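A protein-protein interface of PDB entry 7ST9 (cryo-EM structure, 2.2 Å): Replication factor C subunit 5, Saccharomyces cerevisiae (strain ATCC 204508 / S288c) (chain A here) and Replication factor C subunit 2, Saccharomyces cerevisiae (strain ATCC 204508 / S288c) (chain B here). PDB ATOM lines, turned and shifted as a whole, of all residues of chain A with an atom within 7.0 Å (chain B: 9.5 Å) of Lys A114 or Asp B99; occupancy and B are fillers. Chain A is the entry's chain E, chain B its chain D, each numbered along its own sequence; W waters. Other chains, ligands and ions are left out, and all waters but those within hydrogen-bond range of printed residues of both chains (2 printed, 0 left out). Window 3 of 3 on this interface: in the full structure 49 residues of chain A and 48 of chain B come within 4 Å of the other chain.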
ATOM      1  N   ARG A 106      12.299  18.962 -13.091  1.00  0.00           N
ATOM      2  CA  ARG A 106      11.403  19.185 -14.221  1.00  0.00           C
ATOM      3  C   ARG A 106      12.005  18.644 -15.512  1.00  0.00           C
ATOM      4  O   ARG A 106      11.293  18.073 -16.347  1.00  0.00           O
ATOM      5  CB  ARG A 106      11.077  20.675 -14.351  1.00  0.00           C
ATOM      6  CG  ARG A 106      12.182  21.532 -14.960  1.00  0.00           C
ATOM      7  CD  ARG A 106      11.722  22.969 -15.148  1.00  0.00           C
ATOM      8  NE  ARG A 106      11.476  23.284 -16.551  1.00  0.00           N
ATOM      9  CZ  ARG A 106      10.620  24.200 -16.982  1.00  0.00           C
ATOM     10  NH1 ARG A 106       9.905  24.932 -16.141  1.00  0.00           N
ATOM     11  NH2 ARG A 106      10.476  24.390 -18.291  1.00  0.00           N
ATOM     12  N   VAL A 108      13.790  16.032 -15.903  1.00  0.00           N
ATOM     13  CA  VAL A 108      13.513  14.598 -15.935  1.00  0.00           C
ATOM     14  C   VAL A 108      12.105  14.346 -16.453  1.00  0.00           C
ATOM     15  O   VAL A 108      11.872  13.418 -17.237  1.00  0.00           O
ATOM     16  CB  VAL A 108      13.714  13.983 -14.537  1.00  0.00           C
ATOM     17  CG1 VAL A 108      13.336  12.508 -14.543  1.00  0.00           C
ATOM     18  CG2 VAL A 108      15.142  14.171 -14.078  1.00  0.00           C
ATOM     19  N   ILE A 109      11.144  15.164 -16.022  1.00  0.00           N
ATOM     20  CA  ILE A 109       9.773  14.989 -16.485  1.00  0.00           C
ATOM     21  C   ILE A 109       9.662  15.338 -17.963  1.00  0.00           C
ATOM     22  O   ILE A 109       8.924  14.688 -18.713  1.00  0.00           O
ATOM     23  CB  ILE A 109       8.812  15.835 -15.630  1.00  0.00           C
ATOM     24  CG1 ILE A 109       9.002  15.532 -14.139  1.00  0.00           C
ATOM     25  CG2 ILE A 109       7.368  15.588 -16.046  1.00  0.00           C
ATOM     26  CD1 ILE A 109       8.950  14.057 -13.786  1.00  0.00           C
ATOM     27  N   GLN A 110      10.392  16.364 -18.407  1.00  0.00           N
ATOM     28  CA  GLN A 110      10.209  16.863 -19.765  1.00  0.00           C
ATOM     29  C   GLN A 110      10.869  15.959 -20.798  1.00  0.00           C
ATOM     30  O   GLN A 110      10.348  15.800 -21.907  1.00  0.00           O
ATOM     31  CB  GLN A 110      10.757  18.286 -19.875  1.00  0.00           C
ATOM     32  CG  GLN A 110       9.863  19.335 -19.234  1.00  0.00           C
ATOM     33  CD  GLN A 110      10.363  20.747 -19.460  1.00  0.00           C
ATOM     34  OE1 GLN A 110      11.566  20.982 -19.569  1.00  0.00           O
ATOM     35  NE2 GLN A 110       9.439  21.698 -19.530  1.00  0.00           N
ATOM     36  N   GLU A 111      12.012  15.361 -20.461  1.00  0.00           N
ATOM     37  CA  GLU A 111      12.786  14.571 -21.414  1.00  0.00           C
ATOM     38  C   GLU A 111      12.570  13.071 -21.235  1.00  0.00           C
ATOM     39  O   GLU A 111      12.146  12.388 -22.171  1.00  0.00           O
ATOM     40  CB  GLU A 111      14.275  14.914 -21.284  1.00  0.00           C
ATOM     41  CG  GLU A 111      14.549  16.396 -21.091  1.00  0.00           C
ATOM     42  CD  GLU A 111      15.751  16.874 -21.879  1.00  0.00           C
ATOM     43  OE1 GLU A 111      15.610  17.107 -23.096  1.00  0.00           O
ATOM     44  OE2 GLU A 111      16.837  17.016 -21.280  1.00  0.00           O
ATOM     45  N   LEU A 112      12.851  12.544 -20.043  1.00  0.00           N
ATOM     46  CA  LEU A 112      12.797  11.099 -19.849  1.00  0.00           C
ATOM     47  C   LEU A 112      11.360  10.595 -19.867  1.00  0.00           C
ATOM     48  O   LEU A 112      10.958   9.854 -20.773  1.00  0.00           O
ATOM     49  CB  LEU A 112      13.486  10.725 -18.535  1.00  0.00           C
ATOM     50  CG  LEU A 112      13.293   9.285 -18.052  1.00  0.00           C
ATOM     51  CD1 LEU A 112      13.623   8.292 -19.156  1.00  0.00           C
ATOM     52  CD2 LEU A 112      14.139   9.015 -16.819  1.00  0.00           C
ATOM     53  N   LEU A 113      10.554  11.024 -18.892  1.00  0.00           N
ATOM     54  CA  LEU A 113       9.210  10.474 -18.753  1.00  0.00           C
ATOM     55  C   LEU A 113       8.414  10.652 -20.037  1.00  0.00           C
ATOM     56  O   LEU A 113       7.799   9.702 -20.537  1.00  0.00           O
ATOM     57  CB  LEU A 113       8.493  11.137 -17.576  1.00  0.00           C
ATOM     58  CG  LEU A 113       7.157  10.503 -17.178  1.00  0.00           C
ATOM     59  CD1 LEU A 113       7.355   9.073 -16.695  1.00  0.00           C
ATOM     60  CD2 LEU A 113       6.468  11.337 -16.114  1.00  0.00           C
ATOM     61  N   LYS A 114       8.438  11.860 -20.605  1.00  0.00           N
ATOM     62  CA  LYS A 114       7.727  12.100 -21.855  1.00  0.00           C
ATOM     63  C   LYS A 114       8.122  11.070 -22.904  1.00  0.00           C
ATOM     64  O   LYS A 114       7.262  10.441 -23.532  1.00  0.00           O
ATOM     65  CB  LYS A 114       8.007  13.518 -22.358  1.00  0.00           C
ATOM     66  CG  LYS A 114       7.084  13.964 -23.481  1.00  0.00           C
ATOM     67  CD  LYS A 114       7.143  15.468 -23.694  1.00  0.00           C
ATOM     68  CE  LYS A 114       6.142  15.919 -24.746  1.00  0.00           C
ATOM     69  NZ  LYS A 114       6.077  17.402 -24.861  1.00  0.00           N
ATOM     70  N   GLU A 115       9.427  10.852 -23.078  1.00  0.00           N
ATOM     71  CA  GLU A 115       9.876   9.862 -24.049  1.00  0.00           C
ATOM     72  C   GLU A 115       9.301   8.492 -23.719  1.00  0.00           C
ATOM     73  O   GLU A 115       8.768   7.800 -24.596  1.00  0.00           O
ATOM     74  CB  GLU A 115      11.403   9.814 -24.086  1.00  0.00           C
ATOM     75  CG  GLU A 115      12.035  10.973 -24.836  1.00  0.00           C
ATOM     76  CD  GLU A 115      13.500  11.160 -24.490  1.00  0.00           C
ATOM     77  OE1 GLU A 115      14.248  10.161 -24.512  1.00  0.00           O
ATOM     78  OE2 GLU A 115      13.900  12.306 -24.194  1.00  0.00           O
ATOM     79  N   VAL A 116       9.359   8.103 -22.443  1.00  0.00           N
ATOM     80  CA  VAL A 116       8.788   6.823 -22.040  1.00  0.00           C
ATOM     81  C   VAL A 116       7.308   6.784 -22.381  1.00  0.00           C
ATOM     82  O   VAL A 116       6.779   5.753 -22.813  1.00  0.00           O
ATOM     83  CB  VAL A 116       9.031   6.577 -20.538  1.00  0.00           C
ATOM     84  CG1 VAL A 116       8.236   5.371 -20.059  1.00  0.00           C
ATOM     85  CG2 VAL A 116      10.514   6.389 -20.262  1.00  0.00           C
ATOM     86  N   ALA A 117       6.613   7.909 -22.193  1.00  0.00           N
ATOM     87  CA  ALA A 117       5.195   7.956 -22.526  1.00  0.00           C
ATOM     88  C   ALA A 117       4.970   7.895 -24.030  1.00  0.00           C
ATOM     89  O   ALA A 117       3.948   7.367 -24.479  1.00  0.00           O
ATOM     90  CB  ALA A 117       4.565   9.222 -21.946  1.00  0.00           C
ATOM     91  N   GLN A 118       5.907   8.425 -24.822  1.00  0.00           N
ATOM     92  CA  GLN A 118       5.697   8.505 -26.263  1.00  0.00           C
ATOM     93  C   GLN A 118       5.996   7.187 -26.967  1.00  0.00           C
ATOM     94  O   GLN A 118       5.383   6.891 -27.998  1.00  0.00           O
ATOM     95  CB  GLN A 118       6.559   9.621 -26.854  1.00  0.00           C
ATOM     96  CG  GLN A 118       5.936  11.004 -26.736  1.00  0.00           C
ATOM     97  CD  GLN A 118       6.897  12.113 -27.114  1.00  0.00           C
ATOM     98  OE1 GLN A 118       8.091  11.881 -27.296  1.00  0.00           O
ATOM     99  NE2 GLN A 118       6.378  13.328 -27.235  1.00  0.00           N
ATOM    100  N   MET A 119       6.918   6.391 -26.434  1.00  0.00           N
ATOM    101  CA  MET A 119       7.317   5.136 -27.068  1.00  0.00           C
ATOM    102  C   MET A 119       6.321   4.052 -26.675  1.00  0.00           C
ATOM    103  O   MET A 119       6.346   3.544 -25.554  1.00  0.00           O
ATOM    104  CB  MET A 119       8.734   4.759 -26.656  1.00  0.00           C
ATOM    105  CG  MET A 119       9.410   3.772 -27.595  1.00  0.00           C
ATOM    106  SD  MET A 119      11.172   3.591 -27.264  1.00  0.00           S
ATOM    107  CE  MET A 119      11.146   3.015 -25.569  1.00  0.00           C
ATOM    108  N   ALA A 153       4.451  19.967 -15.666  1.00  0.00           N
ATOM    109  CA  ALA A 153       4.865  19.224 -16.853  1.00  0.00           C
ATOM    110  C   ALA A 153       4.269  17.822 -16.877  1.00  0.00           C
ATOM    111  O   ALA A 153       4.118  17.230 -17.951  1.00  0.00           O
ATOM    112  CB  ALA A 153       6.391  19.150 -16.919  1.00  0.00           C
ATOM    113  N   THR A 157       1.360  14.987 -20.101  1.00  0.00           N
ATOM    114  CA  THR A 157       1.957  13.670 -20.293  1.00  0.00           C
ATOM    115  C   THR A 157       1.043  12.580 -19.750  1.00  0.00           C
ATOM    116  O   THR A 157       0.822  11.557 -20.410  1.00  0.00           O
ATOM    117  CB  THR A 157       3.328  13.607 -19.618  1.00  0.00           C
ATOM    118  OG1 THR A 157       4.192  14.598 -20.190  1.00  0.00           O
ATOM    119  CG2 THR A 157       3.953  12.231 -19.797  1.00  0.00           C
ATOM    120  N   LYS A 160      -2.525  12.824 -22.294  1.00  0.00           N
ATOM    121  CA  LYS A 160      -2.492  12.457 -23.708  1.00  0.00           C
ATOM    122  C   LYS A 160      -2.047  11.012 -23.908  1.00  0.00           C
ATOM    123  O   LYS A 160      -2.620  10.289 -24.732  1.00  0.00           O
ATOM    124  CB  LYS A 160      -1.567  13.406 -24.469  1.00  0.00           C
ATOM    125  CG  LYS A 160      -1.964  13.626 -25.919  1.00  0.00           C
ATOM    126  CD  LYS A 160      -1.274  14.846 -26.508  1.00  0.00           C
ATOM    127  CE  LYS A 160       0.162  14.540 -26.896  1.00  0.00           C
ATOM    128  NZ  LYS A 160       0.241  13.761 -28.163  1.00  0.00           N
ATOM    129  N   TYR A 161      -1.026  10.573 -23.173  1.00  0.00           N
ATOM    130  CA  TYR A 161      -0.422   9.261 -23.376  1.00  0.00           C
ATOM    131  C   TYR A 161      -0.912   8.232 -22.364  1.00  0.00           C
ATOM    132  O   TYR A 161      -0.159   7.330 -21.982  1.00  0.00           O
ATOM    133  CB  TYR A 161       1.101   9.377 -23.329  1.00  0.00           C
ATOM    134  CG  TYR A 161       1.659  10.305 -24.382  1.00  0.00           C
ATOM    135  CD1 TYR A 161       1.632   9.957 -25.726  1.00  0.00           C
ATOM    136  CD2 TYR A 161       2.200  11.535 -24.036  1.00  0.00           C
ATOM    137  CE1 TYR A 161       2.134  10.802 -26.692  1.00  0.00           C
ATOM    138  CE2 TYR A 161       2.705  12.388 -24.996  1.00  0.00           C
ATOM    139  CZ  TYR A 161       2.669  12.016 -26.322  1.00  0.00           C
ATOM    140  OH  TYR A 161       3.171  12.863 -27.283  1.00  0.00           O
ATOM    141  N   ILE A 165       1.080   4.594 -20.758  1.00  0.00           N
ATOM    142  CA  ILE A 165       1.720   4.788 -19.462  1.00  0.00           C
ATOM    143  C   ILE A 165       0.659   4.908 -18.379  1.00  0.00           C
ATOM    144  O   ILE A 165      -0.425   5.453 -18.599  1.00  0.00           O
ATOM    145  CB  ILE A 165       2.639   6.034 -19.468  1.00  0.00           C
ATOM    146  CG1 ILE A 165       3.619   5.976 -18.296  1.00  0.00           C
ATOM    147  CG2 ILE A 165       1.812   7.310 -19.406  1.00  0.00           C
ATOM    148  CD1 ILE A 165       4.691   7.044 -18.347  1.00  0.00           C
ATOM    149  N   LEU B  93      -0.991  23.958 -33.751  1.00  0.00           N
ATOM    150  CA  LEU B  93       0.280  23.842 -33.041  1.00  0.00           C
ATOM    151  C   LEU B  93      -0.006  23.914 -31.547  1.00  0.00           C
ATOM    152  O   LEU B  93      -0.421  24.962 -31.045  1.00  0.00           O
ATOM    153  CB  LEU B  93       1.265  24.935 -33.460  1.00  0.00           C
ATOM    154  CG  LEU B  93       2.512  25.067 -32.579  1.00  0.00           C
ATOM    155  CD1 LEU B  93       3.230  23.731 -32.447  1.00  0.00           C
ATOM    156  CD2 LEU B  93       3.457  26.124 -33.126  1.00  0.00           C
ATOM    157  N   GLU B  94       0.223  22.812 -30.838  1.00  0.00           N
ATOM    158  CA  GLU B  94      -0.080  22.705 -29.416  1.00  0.00           C
ATOM    159  C   GLU B  94       1.209  22.682 -28.608  1.00  0.00           C
ATOM    160  O   GLU B  94       2.131  21.921 -28.921  1.00  0.00           O
ATOM    161  CB  GLU B  94      -0.901  21.445 -29.128  1.00  0.00           C
ATOM    162  CG  GLU B  94      -1.851  21.570 -27.943  1.00  0.00           C
ATOM    163  CD  GLU B  94      -1.230  21.119 -26.635  1.00  0.00           C
ATOM    164  OE1 GLU B  94       0.015  21.063 -26.547  1.00  0.00           O
ATOM    165  OE2 GLU B  94      -1.988  20.818 -25.689  1.00  0.00           O
ATOM    166  N   LEU B  95       1.268  23.515 -27.570  1.00  0.00           N
ATOM    167  CA  LEU B  95       2.370  23.525 -26.618  1.00  0.00           C
ATOM    168  C   LEU B  95       1.801  23.598 -25.209  1.00  0.00           C
ATOM    169  O   LEU B  95       0.817  24.303 -24.967  1.00  0.00           O
ATOM    170  CB  LEU B  95       3.318  24.704 -26.863  1.00  0.00           C
ATOM    171  CG  LEU B  95       4.068  24.703 -28.198  1.00  0.00           C
ATOM    172  CD1 LEU B  95       4.835  26.003 -28.377  1.00  0.00           C
ATOM    173  CD2 LEU B  95       5.005  23.509 -28.293  1.00  0.00           C
ATOM    174  N   ASN B  96       2.420  22.871 -24.283  1.00  0.00           N
ATOM    175  CA  ASN B  96       1.938  22.799 -22.909  1.00  0.00           C
ATOM    176  C   ASN B  96       3.143  22.836 -21.972  1.00  0.00           C
ATOM    177  O   ASN B  96       4.277  23.080 -22.392  1.00  0.00           O
ATOM    178  CB  ASN B  96       1.071  21.548 -22.713  1.00  0.00           C
ATOM    179  CG  ASN B  96       1.747  20.286 -23.209  1.00  0.00           C
ATOM    180  OD1 ASN B  96       2.896  20.009 -22.867  1.00  0.00           O
ATOM    181  ND2 ASN B  96       1.036  19.514 -24.022  1.00  0.00           N
ATOM    182  N   ALA B  97       2.886  22.594 -20.683  1.00  0.00           N
ATOM    183  CA  ALA B  97       3.941  22.702 -19.680  1.00  0.00           C
ATOM    184  C   ALA B  97       5.037  21.663 -19.889  1.00  0.00           C
ATOM    185  O   ALA B  97       6.186  21.889 -19.495  1.00  0.00           O
ATOM    186  CB  ALA B  97       3.345  22.566 -18.279  1.00  0.00           C
ATOM    187  N   SER B  98       4.709  20.522 -20.498  1.00  0.00           N
ATOM    188  CA  SER B  98       5.717  19.498 -20.739  1.00  0.00           C
ATOM    189  C   SER B  98       6.700  19.887 -21.835  1.00  0.00           C
ATOM    190  O   SER B  98       7.707  19.195 -22.012  1.00  0.00           O
ATOM    191  CB  SER B  98       5.046  18.169 -21.097  1.00  0.00           C
ATOM    192  OG  SER B  98       4.402  18.236 -22.356  1.00  0.00           O
ATOM    193  N   ASP B  99       6.437  20.966 -22.566  1.00  0.00           N
ATOM    194  CA  ASP B  99       7.315  21.440 -23.624  1.00  0.00           C
ATOM    195  C   ASP B  99       8.151  22.619 -23.139  1.00  0.00           C
ATOM    196  O   ASP B  99       7.780  23.336 -22.208  1.00  0.00           O
ATOM    197  CB  ASP B  99       6.502  21.857 -24.853  1.00  0.00           C
ATOM    198  CG  ASP B  99       5.772  20.697 -25.492  1.00  0.00           C
ATOM    199  OD1 ASP B  99       6.389  19.624 -25.660  1.00  0.00           O
ATOM    200  OD2 ASP B  99       4.579  20.856 -25.826  1.00  0.00           O
ATOM    201  N   GLU B 100       9.295  22.810 -23.790  1.00  0.00           N
ATOM    202  CA  GLU B 100      10.110  23.987 -23.527  1.00  0.00           C
ATOM    203  C   GLU B 100       9.444  25.214 -24.140  1.00  0.00           C
ATOM    204  O   GLU B 100       9.092  25.213 -25.324  1.00  0.00           O
ATOM    205  CB  GLU B 100      11.514  23.799 -24.100  1.00  0.00           C
ATOM    206  CG  GLU B 100      12.619  24.385 -23.234  1.00  0.00           C
ATOM    207  CD  GLU B 100      13.139  23.408 -22.195  1.00  0.00           C
ATOM    208  OE1 GLU B 100      12.840  22.199 -22.300  1.00  0.00           O
ATOM    209  OE2 GLU B 100      13.852  23.850 -21.270  1.00  0.00           O
ATOM    210  N   ARG B 101       9.261  26.255 -23.333  1.00  0.00           N
ATOM    211  CA  ARG B 101       8.540  27.452 -23.759  1.00  0.00           C
ATOM    212  C   ARG B 101       9.265  28.707 -23.281  1.00  0.00           C
ATOM    213  O   ARG B 101       8.659  29.650 -22.770  1.00  0.00           O
ATOM    214  CB  ARG B 101       7.099  27.415 -23.254  1.00  0.00           C
ATOM    215  CG  ARG B 101       6.285  26.264 -23.821  1.00  0.00           C
ATOM    216  CD  ARG B 101       4.808  26.406 -23.508  1.00  0.00           C
ATOM    217  NE  ARG B 101       4.529  26.256 -22.085  1.00  0.00           N
ATOM    218  CZ  ARG B 101       3.312  26.201 -21.562  1.00  0.00           C
ATOM    219  NH1 ARG B 101       2.229  26.277 -22.319  1.00  0.00           N
ATOM    220  NH2 ARG B 101       3.178  26.061 -20.246  1.00  0.00           N
ATOM    221  N   GLY B 102      10.581  28.731 -23.452  1.00  0.00           N
ATOM    222  CA  GLY B 102      11.364  29.900 -23.115  1.00  0.00           C
ATOM    223  C   GLY B 102      11.160  31.021 -24.119  1.00  0.00           C
ATOM    224  O   GLY B 102      10.458  30.893 -25.124  1.00  0.00           O
ATOM    225  N   ILE B 105      12.068  30.137 -27.623  1.00  0.00           N
ATOM    226  CA  ILE B 105      11.049  29.322 -28.277  1.00  0.00           C
ATOM    227  C   ILE B 105       9.919  30.206 -28.791  1.00  0.00           C
ATOM    228  O   ILE B 105       9.495  30.089 -29.946  1.00  0.00           O
ATOM    229  CB  ILE B 105      10.523  28.241 -27.314  1.00  0.00           C
ATOM    230  CG1 ILE B 105      11.659  27.316 -26.864  1.00  0.00           C
ATOM    231  CG2 ILE B 105       9.403  27.444 -27.967  1.00  0.00           C
ATOM    232  CD1 ILE B 105      12.329  26.551 -27.989  1.00  0.00           C
ATOM    233  N   LYS B 109       9.975  29.522 -32.729  1.00  0.00           N
ATOM    234  CA  LYS B 109       9.094  28.461 -33.209  1.00  0.00           C
ATOM    235  C   LYS B 109       7.651  28.941 -33.319  1.00  0.00           C
ATOM    236  O   LYS B 109       6.995  28.743 -34.352  1.00  0.00           O
ATOM    237  CB  LYS B 109       9.194  27.251 -32.276  1.00  0.00           C
ATOM    238  CG  LYS B 109       8.079  26.228 -32.428  1.00  0.00           C
ATOM    239  CD  LYS B 109       8.361  24.990 -31.592  1.00  0.00           C
ATOM    240  CE  LYS B 109       7.207  24.002 -31.637  1.00  0.00           C
ATOM    241  NZ  LYS B 109       7.480  22.865 -32.557  1.00  0.00           N
ATOM    242  N   VAL B 110       7.144  29.579 -32.262  1.00  0.00           N
ATOM    243  CA  VAL B 110       5.781  30.095 -32.289  1.00  0.00           C
ATOM    244  C   VAL B 110       5.643  31.153 -33.375  1.00  0.00           C
ATOM    245  O   VAL B 110       4.653  31.179 -34.116  1.00  0.00           O
ATOM    246  CB  VAL B 110       5.392  30.649 -30.905  1.00  0.00           C
ATOM    247  CG1 VAL B 110       3.950  31.134 -30.907  1.00  0.00           C
ATOM    248  CG2 VAL B 110       5.603  29.594 -29.828  1.00  0.00           C
ATOM    249  N   ILE B 138      -2.313  26.660 -29.720  1.00  0.00           N
ATOM    250  CA  ILE B 138      -2.838  26.397 -28.387  1.00  0.00           C
ATOM    251  C   ILE B 138      -1.670  26.392 -27.413  1.00  0.00           C
ATOM    252  O   ILE B 138      -0.686  25.669 -27.616  1.00  0.00           O
ATOM    253  CB  ILE B 138      -3.603  25.062 -28.335  1.00  0.00           C
ATOM    254  CG1 ILE B 138      -4.723  25.043 -29.378  1.00  0.00           C
ATOM    255  CG2 ILE B 138      -4.169  24.823 -26.939  1.00  0.00           C
ATOM    256  CD1 ILE B 138      -5.283  23.664 -29.642  1.00  0.00           C
ATOM    257  N   LEU B 139      -1.768  27.213 -26.373  1.00  0.00           N
ATOM    258  CA  LEU B 139      -0.772  27.276 -25.307  1.00  0.00           C
ATOM    259  C   LEU B 139      -1.462  26.818 -24.026  1.00  0.00           C
ATOM    260  O   LEU B 139      -1.963  27.633 -23.249  1.00  0.00           O
ATOM    261  CB  LEU B 139      -0.189  28.687 -25.175  1.00  0.00           C
ATOM    262  CG  LEU B 139       0.500  29.241 -26.426  1.00  0.00           C
ATOM    263  CD1 LEU B 139       1.021  30.651 -26.185  1.00  0.00           C
ATOM    264  CD2 LEU B 139       1.628  28.325 -26.878  1.00  0.00           C
ATOM    265  N   ASP B 140      -1.490  25.505 -23.815  1.00  0.00           N
ATOM    266  CA  ASP B 140      -2.076  24.954 -22.604  1.00  0.00           C
ATOM    267  C   ASP B 140      -1.164  25.218 -21.412  1.00  0.00           C
ATOM    268  O   ASP B 140       0.060  25.291 -21.542  1.00  0.00           O
ATOM    269  CB  ASP B 140      -2.318  23.451 -22.762  1.00  0.00           C
ATOM    270  CG  ASP B 140      -3.547  22.972 -22.008  1.00  0.00           C
ATOM    271  OD1 ASP B 140      -4.033  23.704 -21.122  1.00  0.00           O
ATOM    272  OD2 ASP B 140      -4.028  21.858 -22.305  1.00  0.00           O
ATOM    273  N   GLU B 141      -1.775  25.364 -20.237  1.00  0.00           N
ATOM    274  CA  GLU B 141      -1.038  25.704 -19.022  1.00  0.00           C
ATOM    275  C   GLU B 141      -0.196  26.958 -19.241  1.00  0.00           C
ATOM    276  O   GLU B 141       0.971  27.029 -18.852  1.00  0.00           O
ATOM    277  CB  GLU B 141      -0.168  24.531 -18.564  1.00  0.00           C
ATOM    278  CG  GLU B 141      -0.960  23.361 -17.992  1.00  0.00           C
ATOM    279  CD  GLU B 141      -1.055  22.179 -18.942  1.00  0.00           C
ATOM    280  OE1 GLU B 141      -0.783  22.349 -20.149  1.00  0.00           O
ATOM    281  OE2 GLU B 141      -1.409  21.075 -18.480  1.00  0.00           O
ATOM    282  N   SER B 144       2.120  28.843 -16.653  1.00  0.00           N
ATOM    283  CA  SER B 144       3.474  28.432 -16.301  1.00  0.00           C
ATOM    284  C   SER B 144       4.547  29.196 -17.067  1.00  0.00           C
ATOM    285  O   SER B 144       5.727  29.087 -16.718  1.00  0.00           O
ATOM    286  CB  SER B 144       3.651  26.930 -16.552  1.00  0.00           C
ATOM    287  OG  SER B 144       2.582  26.187 -15.991  1.00  0.00           O
ATOM    288  N   MET B 145       4.175  29.957 -18.093  1.00  0.00           N
ATOM    289  CA  MET B 145       5.149  30.694 -18.886  1.00  0.00           C
ATOM    290  C   MET B 145       5.607  31.948 -18.148  1.00  0.00           C
ATOM    291  O   MET B 145       4.854  32.559 -17.385  1.00  0.00           O
ATOM    292  CB  MET B 145       4.554  31.077 -20.241  1.00  0.00           C
ATOM    293  CG  MET B 145       4.602  29.959 -21.271  1.00  0.00           C
ATOM    294  SD  MET B 145       3.753  30.369 -22.809  1.00  0.00           S
ATOM    295  CE  MET B 145       4.728  31.758 -23.382  1.00  0.00           C
HETATM  296  O   HOH W   1       1.942  19.377 -19.048  1.00  0.00           O
HETATM  297  O   HOH W   2       9.756  26.572 -20.689  1.00  0.00           O
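O of Ala B97 lies within hydrogen-bond range of NE2 of Gln A110 (3.3 Å). The side-chain hydroxyl (OG) of Ser B98 lies within hydrogen-bond range of the side-chain amino group (NZ) of Lys A114, 3.1 Å away. NZ of Lys A114 lies within salt-bridge range of OD2 of Asp B99 (3.9 Å). OE1 of Glu B100 lies close to OE1 of Gln A110.
The side-chain amide oxygen (OD1) of Asn B96 is in hydrogen-bond range of the backbone NH (N) of Ser B98, at 3.0 Å. OD2 of Asp B99 sits at hydrogen-bond distance from N of Asn B96 (3.3 Å). NE2 of Gln A110 lies close to NH2 of Arg A106 (3.1 Å). O of Ile A109 lies within hydrogen-bond range of N of Lys A114 (3.4 Å). The backbone carbonyl oxygen (O) of Ala A153 is in hydrogen-bond range of the side-chain hydroxyl (OG1) of Thr A157, at 3.5 Å.
Among the printed residues, merely in contact across the chains: Ala A153 with Ser B98, Gln A110 with Ser B98, Gln A110 with Asp B99, Ala A153 with Ala B97 and Thr A157 with Ser B98.
No residue of chain B comes within 4 Å of Leu A113. Of the printed residues of chain B, Thr A157 touches Ser B98. Lys A160 touches none of the printed residues of chain B. Of the printed residues of chain A, Ala B97 touches Gln A110 and Ala A153. Printed residues of chain A within 4 Å of Ser B98: Gln A110 (3.5 Å), Lys A114 (3.1 Å), Ala A153 (3.4 Å) and Thr A157 (3.8 Å). Of chain A, only Gln A110 and Lys A114 come within 4 Å of Asp B99. Ile B105 touches none of the printed residues of chain A. The nearest residue of chain B that does not touch Lys A114 is Asn B96 (4.6 Å). The nearest residue of chain A that does not touch Asp B99 is Arg A106 (4.9 Å).
Of the 18 printed residues of chain A, 4 touch a printed residue of chain B. Printed residues of chain B that touch a printed residue of chain A: Ala B97, Ser B98, Asp B99 and Glu B100. Hydrophobic or aromatic side chains of chain B within 4 Å of the printed part of chain A: Ala B97. Among the printed residues, Asp or Glu carboxylates within 4 Å of a Lys or Arg side-chain nitrogen of the other chain: Lys A114 with Asp B99 (2.4 Å).
Water W2 bridges N of Arg B101 (2.7 Å) and NH2 of Arg A106 (3.3 Å). Water W1 bridges the backbone carbonyl oxygen of Ala A153 (3.2 Å) and the backbone NH of Ser B98 (3.3 Å).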
